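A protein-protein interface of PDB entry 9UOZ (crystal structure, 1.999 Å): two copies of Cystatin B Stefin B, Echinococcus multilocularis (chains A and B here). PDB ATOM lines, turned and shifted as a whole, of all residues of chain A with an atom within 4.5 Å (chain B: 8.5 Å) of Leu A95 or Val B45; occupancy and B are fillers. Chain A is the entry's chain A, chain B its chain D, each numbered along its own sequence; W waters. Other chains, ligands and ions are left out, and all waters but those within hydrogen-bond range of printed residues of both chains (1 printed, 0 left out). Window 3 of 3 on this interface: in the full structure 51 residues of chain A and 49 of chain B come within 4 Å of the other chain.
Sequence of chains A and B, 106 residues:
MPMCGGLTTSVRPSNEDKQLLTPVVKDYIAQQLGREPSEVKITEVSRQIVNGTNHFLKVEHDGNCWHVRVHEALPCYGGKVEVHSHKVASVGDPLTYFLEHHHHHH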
ATOM      1  N   HIS A  55      23.805   3.201  15.815  1.00  0.00           N
ATOM      2  CA  HIS A  55      22.381   3.087  15.596  1.00  0.00           C
ATOM      3  C   HIS A  55      21.788   2.073  16.561  1.00  0.00           C
ATOM      4  O   HIS A  55      22.184   0.906  16.569  1.00  0.00           O
ATOM      5  CB  HIS A  55      22.103   2.588  14.181  1.00  0.00           C
ATOM      6  CG  HIS A  55      22.633   3.427  13.116  1.00  0.00           C
ATOM      7  ND1 HIS A  55      23.874   3.238  12.544  1.00  0.00           N
ATOM      8  CD2 HIS A  55      22.049   4.425  12.467  1.00  0.00           C
ATOM      9  CE1 HIS A  55      24.041   4.163  11.601  1.00  0.00           C
ATOM     10  NE2 HIS A  55      22.945   4.887  11.526  1.00  0.00           N
ATOM     11  N   PHE A  56      20.845   2.540  17.383  1.00  0.00           N
ATOM     12  CA  PHE A  56      20.055   1.623  18.203  1.00  0.00           C
ATOM     13  C   PHE A  56      18.781   1.320  17.443  1.00  0.00           C
ATOM     14  O   PHE A  56      18.090   2.240  17.010  1.00  0.00           O
ATOM     15  CB  PHE A  56      19.887   2.230  19.600  1.00  0.00           C
ATOM     16  CG  PHE A  56      21.205   2.313  20.362  1.00  0.00           C
ATOM     17  CD1 PHE A  56      22.060   3.402  20.179  1.00  0.00           C
ATOM     18  CD2 PHE A  56      21.669   1.239  21.122  1.00  0.00           C
ATOM     19  CE1 PHE A  56      23.305   3.430  20.798  1.00  0.00           C
ATOM     20  CE2 PHE A  56      22.890   1.304  21.755  1.00  0.00           C
ATOM     21  CZ  PHE A  56      23.710   2.387  21.589  1.00  0.00           C
ATOM     22  N   LEU A  57      18.504   0.028  17.239  1.00  0.00           N
ATOM     23  CA  LEU A  57      17.431  -0.414  16.359  1.00  0.00           C
ATOM     24  C   LEU A  57      16.478  -1.307  17.130  1.00  0.00           C
ATOM     25  O   LEU A  57      16.923  -2.153  17.895  1.00  0.00           O
ATOM     26  CB  LEU A  57      17.979  -1.221  15.180  1.00  0.00           C
ATOM     27  CG  LEU A  57      19.125  -0.598  14.382  1.00  0.00           C
ATOM     28  CD1 LEU A  57      19.566  -1.556  13.319  1.00  0.00           C
ATOM     29  CD2 LEU A  57      18.630   0.698  13.787  1.00  0.00           C
ATOM     30  N   LYS A  58      15.184  -1.114  16.896  1.00  0.00           N
ATOM     31  CA  LYS A  58      14.175  -2.104  17.245  1.00  0.00           C
ATOM     32  C   LYS A  58      13.892  -2.963  16.015  1.00  0.00           C
ATOM     33  O   LYS A  58      13.550  -2.424  14.948  1.00  0.00           O
ATOM     34  CB  LYS A  58      12.927  -1.358  17.722  1.00  0.00           C
ATOM     35  CG  LYS A  58      11.864  -2.267  18.322  1.00  0.00           C
ATOM     36  CD  LYS A  58      10.603  -1.579  18.819  1.00  0.00           C
ATOM     37  CE  LYS A  58      10.384  -1.572  20.311  1.00  0.00           C
ATOM     38  NZ  LYS A  58      10.979  -0.421  20.978  1.00  0.00           N
ATOM     39  N   HIS A  67      16.404  -5.472  20.473  1.00  0.00           N
ATOM     40  CA  HIS A  67      17.095  -4.211  20.295  1.00  0.00           C
ATOM     41  C   HIS A  67      18.537  -4.527  19.911  1.00  0.00           C
ATOM     42  O   HIS A  67      19.155  -5.394  20.508  1.00  0.00           O
ATOM     43  CB  HIS A  67      17.055  -3.323  21.543  1.00  0.00           C
ATOM     44  CG  HIS A  67      15.674  -2.827  21.807  1.00  0.00           C
ATOM     45  ND1 HIS A  67      15.336  -2.155  22.959  1.00  0.00           N
ATOM     46  CD2 HIS A  67      14.548  -2.921  21.063  1.00  0.00           C
ATOM     47  CE1 HIS A  67      14.048  -1.863  22.904  1.00  0.00           C
ATOM     48  NE2 HIS A  67      13.546  -2.320  21.779  1.00  0.00           N
ATOM     49  N   ASP A  93       8.881  -1.865  24.786  1.00  0.00           N
ATOM     50  CA  ASP A  93      10.047  -1.359  25.488  1.00  0.00           C
ATOM     51  C   ASP A  93      10.566  -0.104  24.810  1.00  0.00           C
ATOM     52  O   ASP A  93      10.634  -0.073  23.602  1.00  0.00           O
ATOM     53  CB  ASP A  93      11.150  -2.404  25.582  1.00  0.00           C
ATOM     54  CG  ASP A  93      10.963  -3.458  26.669  1.00  0.00           C
ATOM     55  OD1 ASP A  93      10.026  -3.362  27.479  1.00  0.00           O
ATOM     56  OD2 ASP A  93      11.697  -4.457  26.637  1.00  0.00           O
ATOM     57  N   PRO A  94      10.991   0.930  25.572  1.00  0.00           N
ATOM     58  CA  PRO A  94      11.642   2.073  24.950  1.00  0.00           C
ATOM     59  C   PRO A  94      13.005   1.687  24.382  1.00  0.00           C
ATOM     60  O   PRO A  94      13.701   0.821  24.930  1.00  0.00           O
ATOM     61  CB  PRO A  94      11.756   3.105  26.074  1.00  0.00           C
ATOM     62  CG  PRO A  94      11.738   2.248  27.336  1.00  0.00           C
ATOM     63  CD  PRO A  94      10.904   1.028  27.043  1.00  0.00           C
ATOM     64  N   LEU A  95      13.353   2.308  23.253  1.00  0.00           N
ATOM     65  CA  LEU A  95      14.613   2.060  22.585  1.00  0.00           C
ATOM     66  C   LEU A  95      15.648   2.980  23.201  1.00  0.00           C
ATOM     67  O   LEU A  95      15.641   4.169  22.913  1.00  0.00           O
ATOM     68  CB  LEU A  95      14.382   2.366  21.103  1.00  0.00           C
ATOM     69  CG  LEU A  95      15.532   2.049  20.161  1.00  0.00           C
ATOM     70  CD1 LEU A  95      16.022   0.654  20.373  1.00  0.00           C
ATOM     71  CD2 LEU A  95      15.141   2.184  18.708  1.00  0.00           C
ATOM     72  N   THR A  96      16.490   2.445  24.077  1.00  0.00           N
ATOM     73  CA  THR A  96      17.464   3.272  24.775  1.00  0.00           C
ATOM     74  C   THR A  96      18.869   2.711  24.574  1.00  0.00           C
ATOM     75  O   THR A  96      19.038   1.583  24.089  1.00  0.00           O
ATOM     76  CB  THR A  96      17.112   3.373  26.262  1.00  0.00           C
ATOM     77  OG1 THR A  96      17.287   2.073  26.814  1.00  0.00           O
ATOM     78  CG2 THR A  96      15.694   3.871  26.493  1.00  0.00           C
ATOM     79  N   LEU B   7      21.385  10.298  22.602  1.00  0.00           N
ATOM     80  CA  LEU B   7      20.596   9.657  21.559  1.00  0.00           C
ATOM     81  C   LEU B   7      19.569  10.606  20.952  1.00  0.00           C
ATOM     82  O   LEU B   7      18.925  11.354  21.665  1.00  0.00           O
ATOM     83  CB  LEU B   7      19.918   8.409  22.117  1.00  0.00           C
ATOM     84  CG  LEU B   7      20.728   7.109  21.979  1.00  0.00           C
ATOM     85  CD1 LEU B   7      22.094   7.180  22.712  1.00  0.00           C
ATOM     86  CD2 LEU B   7      19.884   5.912  22.359  1.00  0.00           C
ATOM     87  N   THR B   8      19.399  10.544  19.631  1.00  0.00           N
ATOM     88  CA  THR B   8      18.361  11.315  18.970  1.00  0.00           C
ATOM     89  C   THR B   8      16.997  10.706  19.310  1.00  0.00           C
ATOM     90  O   THR B   8      16.888   9.561  19.747  1.00  0.00           O
ATOM     91  CB  THR B   8      18.575  11.347  17.455  1.00  0.00           C
ATOM     92  OG1 THR B   8      18.493   9.988  17.018  1.00  0.00           O
ATOM     93  CG2 THR B   8      19.880  12.015  17.057  1.00  0.00           C
ATOM     94  N   THR B   9      15.956  11.511  19.071  1.00  0.00           N
ATOM     95  CA  THR B   9      14.570  11.091  19.178  1.00  0.00           C
ATOM     96  C   THR B   9      14.324   9.918  18.237  1.00  0.00           C
ATOM     97  O   THR B   9      14.724   9.937  17.084  1.00  0.00           O
ATOM     98  CB  THR B   9      13.683  12.285  18.811  1.00  0.00           C
ATOM     99  OG1 THR B   9      13.940  13.230  19.848  1.00  0.00           O
ATOM    100  CG2 THR B   9      12.202  11.959  18.783  1.00  0.00           C
ATOM    101  N   SER B  10      13.649   8.895  18.758  1.00  0.00           N
ATOM    102  CA  SER B  10      13.283   7.715  17.987  1.00  0.00           C
ATOM    103  C   SER B  10      12.428   8.106  16.788  1.00  0.00           C
ATOM    104  O   SER B  10      11.496   8.887  16.934  1.00  0.00           O
ATOM    105  CB  SER B  10      12.545   6.748  18.842  1.00  0.00           C
ATOM    106  OG  SER B  10      13.411   6.267  19.852  1.00  0.00           O
ATOM    107  N   VAL B  11      12.734   7.529  15.634  1.00  0.00           N
ATOM    108  CA  VAL B  11      11.931   7.715  14.441  1.00  0.00           C
ATOM    109  C   VAL B  11      11.772   6.360  13.756  1.00  0.00           C
ATOM    110  O   VAL B  11      12.480   5.398  14.047  1.00  0.00           O
ATOM    111  CB  VAL B  11      12.580   8.744  13.494  1.00  0.00           C
ATOM    112  CG1 VAL B  11      12.696  10.131  14.118  1.00  0.00           C
ATOM    113  CG2 VAL B  11      13.948   8.315  13.006  1.00  0.00           C
ATOM    114  N   ARG B  12      10.821   6.286  12.830  1.00  0.00           N
ATOM    115  CA  ARG B  12      10.733   5.152  11.917  1.00  0.00           C
ATOM    116  C   ARG B  12      11.892   5.295  10.948  1.00  0.00           C
ATOM    117  O   ARG B  12      12.247   6.417  10.586  1.00  0.00           O
ATOM    118  CB  ARG B  12       9.419   5.080  11.127  1.00  0.00           C
ATOM    119  CG  ARG B  12       8.153   5.120  11.970  1.00  0.00           C
ATOM    120  CD  ARG B  12       8.182   3.950  12.915  1.00  0.00           C
ATOM    121  NE  ARG B  12       7.041   4.040  13.819  1.00  0.00           N
ATOM    122  CZ  ARG B  12       6.925   3.399  14.979  1.00  0.00           C
ATOM    123  NH1 ARG B  12       7.749   2.419  15.324  1.00  0.00           N
ATOM    124  NH2 ARG B  12       5.909   3.668  15.798  1.00  0.00           N
ATOM    125  N   PRO B  13      12.562   4.198  10.539  1.00  0.00           N
ATOM    126  CA  PRO B  13      13.747   4.312   9.704  1.00  0.00           C
ATOM    127  C   PRO B  13      13.415   4.789   8.295  1.00  0.00           C
ATOM    128  O   PRO B  13      12.369   4.424   7.758  1.00  0.00           O
ATOM    129  CB  PRO B  13      14.295   2.890   9.660  1.00  0.00           C
ATOM    130  CG  PRO B  13      13.088   2.030   9.911  1.00  0.00           C
ATOM    131  CD  PRO B  13      12.214   2.810  10.859  1.00  0.00           C
ATOM    132  N   SER B  14      14.322   5.594   7.726  1.00  0.00           N
ATOM    133  CA  SER B  14      14.218   6.041   6.352  1.00  0.00           C
ATOM    134  C   SER B  14      14.557   4.877   5.425  1.00  0.00           C
ATOM    135  O   SER B  14      14.973   3.807   5.879  1.00  0.00           O
ATOM    136  CB  SER B  14      15.161   7.206   6.105  1.00  0.00           C
ATOM    137  OG  SER B  14      16.522   6.759   6.137  1.00  0.00           O
ATOM    138  N   ASP B  17      18.229   4.165   5.719  1.00  0.00           N
ATOM    139  CA  ASP B  17      18.465   3.370   6.914  1.00  0.00           C
ATOM    140  C   ASP B  17      18.196   1.895   6.622  1.00  0.00           C
ATOM    141  O   ASP B  17      19.011   1.041   6.940  1.00  0.00           O
ATOM    142  CB  ASP B  17      17.597   3.813   8.081  1.00  0.00           C
ATOM    143  CG  ASP B  17      17.866   5.205   8.628  1.00  0.00           C
ATOM    144  OD1 ASP B  17      19.007   5.682   8.455  1.00  0.00           O
ATOM    145  OD2 ASP B  17      16.930   5.809   9.209  1.00  0.00           O
ATOM    146  N   LYS B  18      17.040   1.597   6.017  1.00  0.00           N
ATOM    147  CA  LYS B  18      16.649   0.219   5.789  1.00  0.00           C
ATOM    148  C   LYS B  18      17.639  -0.465   4.852  1.00  0.00           C
ATOM    149  O   LYS B  18      17.950  -1.629   5.059  1.00  0.00           O
ATOM    150  CB  LYS B  18      15.219   0.097   5.269  1.00  0.00           C
ATOM    151  CG  LYS B  18      14.160   0.419   6.317  1.00  0.00           C
ATOM    152  CD  LYS B  18      12.758   0.477   5.710  1.00  0.00           C
ATOM    153  CE  LYS B  18      11.793   1.336   6.450  1.00  0.00           C
ATOM    154  NZ  LYS B  18      10.719   1.785   5.556  1.00  0.00           N
ATOM    155  N   LEU B  21      21.121  -0.919   6.866  1.00  0.00           N
ATOM    156  CA  LEU B  21      21.154  -1.637   8.131  1.00  0.00           C
ATOM    157  C   LEU B  21      20.525  -3.021   8.024  1.00  0.00           C
ATOM    158  O   LEU B  21      20.958  -3.932   8.722  1.00  0.00           O
ATOM    159  CB  LEU B  21      20.472  -0.792   9.206  1.00  0.00           C
ATOM    160  CG  LEU B  21      21.174   0.527   9.535  1.00  0.00           C
ATOM    161  CD1 LEU B  21      20.344   1.333  10.520  1.00  0.00           C
ATOM    162  CD2 LEU B  21      22.597   0.313  10.053  1.00  0.00           C
ATOM    163  N   ILE B  42      12.999  -3.464  10.578  1.00  0.00           N
ATOM    164  CA  ILE B  42      13.440  -2.449  11.520  1.00  0.00           C
ATOM    165  C   ILE B  42      12.275  -1.494  11.733  1.00  0.00           C
ATOM    166  O   ILE B  42      11.880  -0.865  10.776  1.00  0.00           O
ATOM    167  CB  ILE B  42      14.703  -1.737  11.006  1.00  0.00           C
ATOM    168  CG1 ILE B  42      15.812  -2.748  10.713  1.00  0.00           C
ATOM    169  CG2 ILE B  42      15.167  -0.652  11.999  1.00  0.00           C
ATOM    170  CD1 ILE B  42      17.044  -2.138  10.093  1.00  0.00           C
ATOM    171  N   THR B  43      11.790  -1.321  12.970  1.00  0.00           N
ATOM    172  CA  THR B  43      10.565  -0.553  13.199  1.00  0.00           C
ATOM    173  C   THR B  43      10.860   0.811  13.812  1.00  0.00           C
ATOM    174  O   THR B  43      10.046   1.697  13.725  1.00  0.00           O
ATOM    175  CB  THR B  43       9.610  -1.343  14.082  1.00  0.00           C
ATOM    176  OG1 THR B  43      10.268  -1.641  15.316  1.00  0.00           O
ATOM    177  CG2 THR B  43       9.184  -2.642  13.416  1.00  0.00           C
ATOM    178  N   GLU B  44      12.040   0.991  14.412  1.00  0.00           N
ATOM    179  CA  GLU B  44      12.353   2.200  15.155  1.00  0.00           C
ATOM    180  C   GLU B  44      13.876   2.328  15.206  1.00  0.00           C
ATOM    181  O   GLU B  44      14.583   1.309  15.324  1.00  0.00           O
ATOM    182  CB  GLU B  44      11.831   2.064  16.587  1.00  0.00           C
ATOM    183  CG  GLU B  44      11.572   3.368  17.320  1.00  0.00           C
ATOM    184  CD  GLU B  44      10.942   3.209  18.706  1.00  0.00           C
ATOM    185  OE1 GLU B  44      10.395   2.173  19.109  1.00  0.00           O
ATOM    186  OE2 GLU B  44      11.015   4.202  19.442  1.00  0.00           O
ATOM    187  N   VAL B  45      14.368   3.568  15.163  1.00  0.00           N
ATOM    188  CA  VAL B  45      15.798   3.833  15.144  1.00  0.00           C
ATOM    189  C   VAL B  45      16.062   5.076  15.983  1.00  0.00           C
ATOM    190  O   VAL B  45      15.303   6.037  15.946  1.00  0.00           O
ATOM    191  CB  VAL B  45      16.377   4.057  13.723  1.00  0.00           C
ATOM    192  CG1 VAL B  45      17.887   4.296  13.756  1.00  0.00           C
ATOM    193  CG2 VAL B  45      16.064   2.906  12.795  1.00  0.00           C
ATOM    194  N   SER B  46      17.188   5.070  16.682  1.00  0.00           N
ATOM    195  CA  SER B  46      17.690   6.200  17.442  1.00  0.00           C
ATOM    196  C   SER B  46      19.208   6.194  17.266  1.00  0.00           C
ATOM    197  O   SER B  46      19.827   5.131  17.297  1.00  0.00           O
ATOM    198  CB  SER B  46      17.270   6.045  18.885  1.00  0.00           C
ATOM    199  OG  SER B  46      17.862   7.025  19.715  1.00  0.00           O
ATOM    200  N   ARG B  47      19.820   7.365  17.065  1.00  0.00           N
ATOM    201  CA  ARG B  47      21.228   7.444  16.689  1.00  0.00           C
ATOM    202  C   ARG B  47      22.026   8.127  17.788  1.00  0.00           C
ATOM    203  O   ARG B  47      21.552   9.049  18.434  1.00  0.00           O
ATOM    204  CB  ARG B  47      21.488   8.319  15.463  1.00  0.00           C
ATOM    205  CG  ARG B  47      20.829   7.839  14.195  1.00  0.00           C
ATOM    206  CD  ARG B  47      20.902   8.845  13.065  1.00  0.00           C
ATOM    207  NE  ARG B  47      20.457   8.113  11.880  1.00  0.00           N
ATOM    208  CZ  ARG B  47      19.241   7.558  11.766  1.00  0.00           C
ATOM    209  NH1 ARG B  47      18.200   8.114  12.371  1.00  0.00           N
ATOM    210  NH2 ARG B  47      19.062   6.497  10.990  1.00  0.00           N
ATOM    211  N   GLN B  48      23.290   7.724  17.918  1.00  0.00           N
ATOM    212  CA  GLN B  48      24.245   8.395  18.778  1.00  0.00           C
ATOM    213  C   GLN B  48      25.520   8.678  17.989  1.00  0.00           C
ATOM    214  O   GLN B  48      26.078   7.780  17.398  1.00  0.00           O
ATOM    215  CB  GLN B  48      24.542   7.414  19.902  1.00  0.00           C
ATOM    216  CG  GLN B  48      25.454   7.998  20.968  1.00  0.00           C
ATOM    217  CD  GLN B  48      26.058   6.961  21.879  1.00  0.00           C
ATOM    218  OE1 GLN B  48      26.310   5.818  21.493  1.00  0.00           O
ATOM    219  NE2 GLN B  48      26.393   7.387  23.079  1.00  0.00           N
HETATM  220  O   HOH W   1      11.337   3.896  21.803  1.00  0.00           O
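The side-chain carboxylate of Glu B44 is in salt-bridge range of the side-chain amino group of Lys A58 (3.3 Å).
The backbone NH (N) of Phe A56 lies within hydrogen-bond range of the backbone carbonyl oxygen (O) of Ser B46.
The backbone carbonyl oxygen of Lys A58 is in hydrogen-bond range of the backbone NH of Thr B43 (2.9 Å).
The backbone carbonyl oxygen of Val B11 sits at hydrogen-bond distance from the backbone NH of Val B45 (2.9 Å).
The guanidinium group (NH1) of Arg B12 is in hydrogen-bond range of the backbone carbonyl oxygen (O) of Thr B43 (2.9 Å).
The backbone NH of Thr B8 sits at hydrogen-bond distance from the backbone carbonyl oxygen of Arg B47 (2.9 Å).
OG of Ser B10 lies close to OE2 of Glu B44, 3.2 Å away.
The backbone carbonyl oxygen (O) of Thr B8 is in hydrogen-bond range of the side-chain hydroxyl (OG) of Ser B46 (2.7 Å).
NZ of Lys A58 lies within hydrogen-bond range of NE2 of His A67 (3.3 Å).
Among the printed residues, merely in contact across the chains: His A55 with Ser B46, His A55 with Arg B47, Phe A56 with Leu B7, Phe A56 with Val B45, Phe A56 with Gln B48, Leu A57 with Leu B21, Leu A57 with Glu B44, Leu A57 with Val B45, Lys A58 with Ile B42, Leu A95 with Glu B44 and Leu A95 with Val B45.
His A67 touches none of the printed residues of chain B.
Leu A95 touches just these residues of chain B: Glu B44 and Val B45.
No residue of chain B comes within 4 Å of Thr A96.
Of the printed residues of chain A, Leu B21 touches Leu A57 (3.7 Å).
Printed residues of chain A within 4 Å of Ile B42: Lys A58 (3.4 Å).
Of the printed residues of chain A, Glu B44 touches Leu A57, Lys A58 and Leu A95.
Val B45 touches just these residues of chain A: Phe A56, Leu A57 and Leu A95.
Of the printed residues of chain A, Arg B47 touches His A55 (3.9 Å).
Of the printed residues of chain A, Gln B48 touches Phe A56 (3.9 Å).
The nearest residue of chain A that does not touch Val B45 is His A55 (4.4 Å).
Of the 18 printed residues of chain B, 9 touch a printed residue of chain A.
Of the 9 printed residues of chain A, 5 touch a printed residue of chain B.
Printed residues of chain A that touch a printed residue of chain B: His A55, Phe A56, Leu A57, Lys A58 and Leu A95.
Among the printed residues, Asp or Glu carboxylates within 4 Å of a Lys or Arg side-chain nitrogen of the other chain: Lys A58 with Glu B44 (3.3 Å).
No position is printed for both chains.
Water W1 bridges the side-chain carboxylate (OE2) of Glu B44 and the backbone NH (N) of Leu A95.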
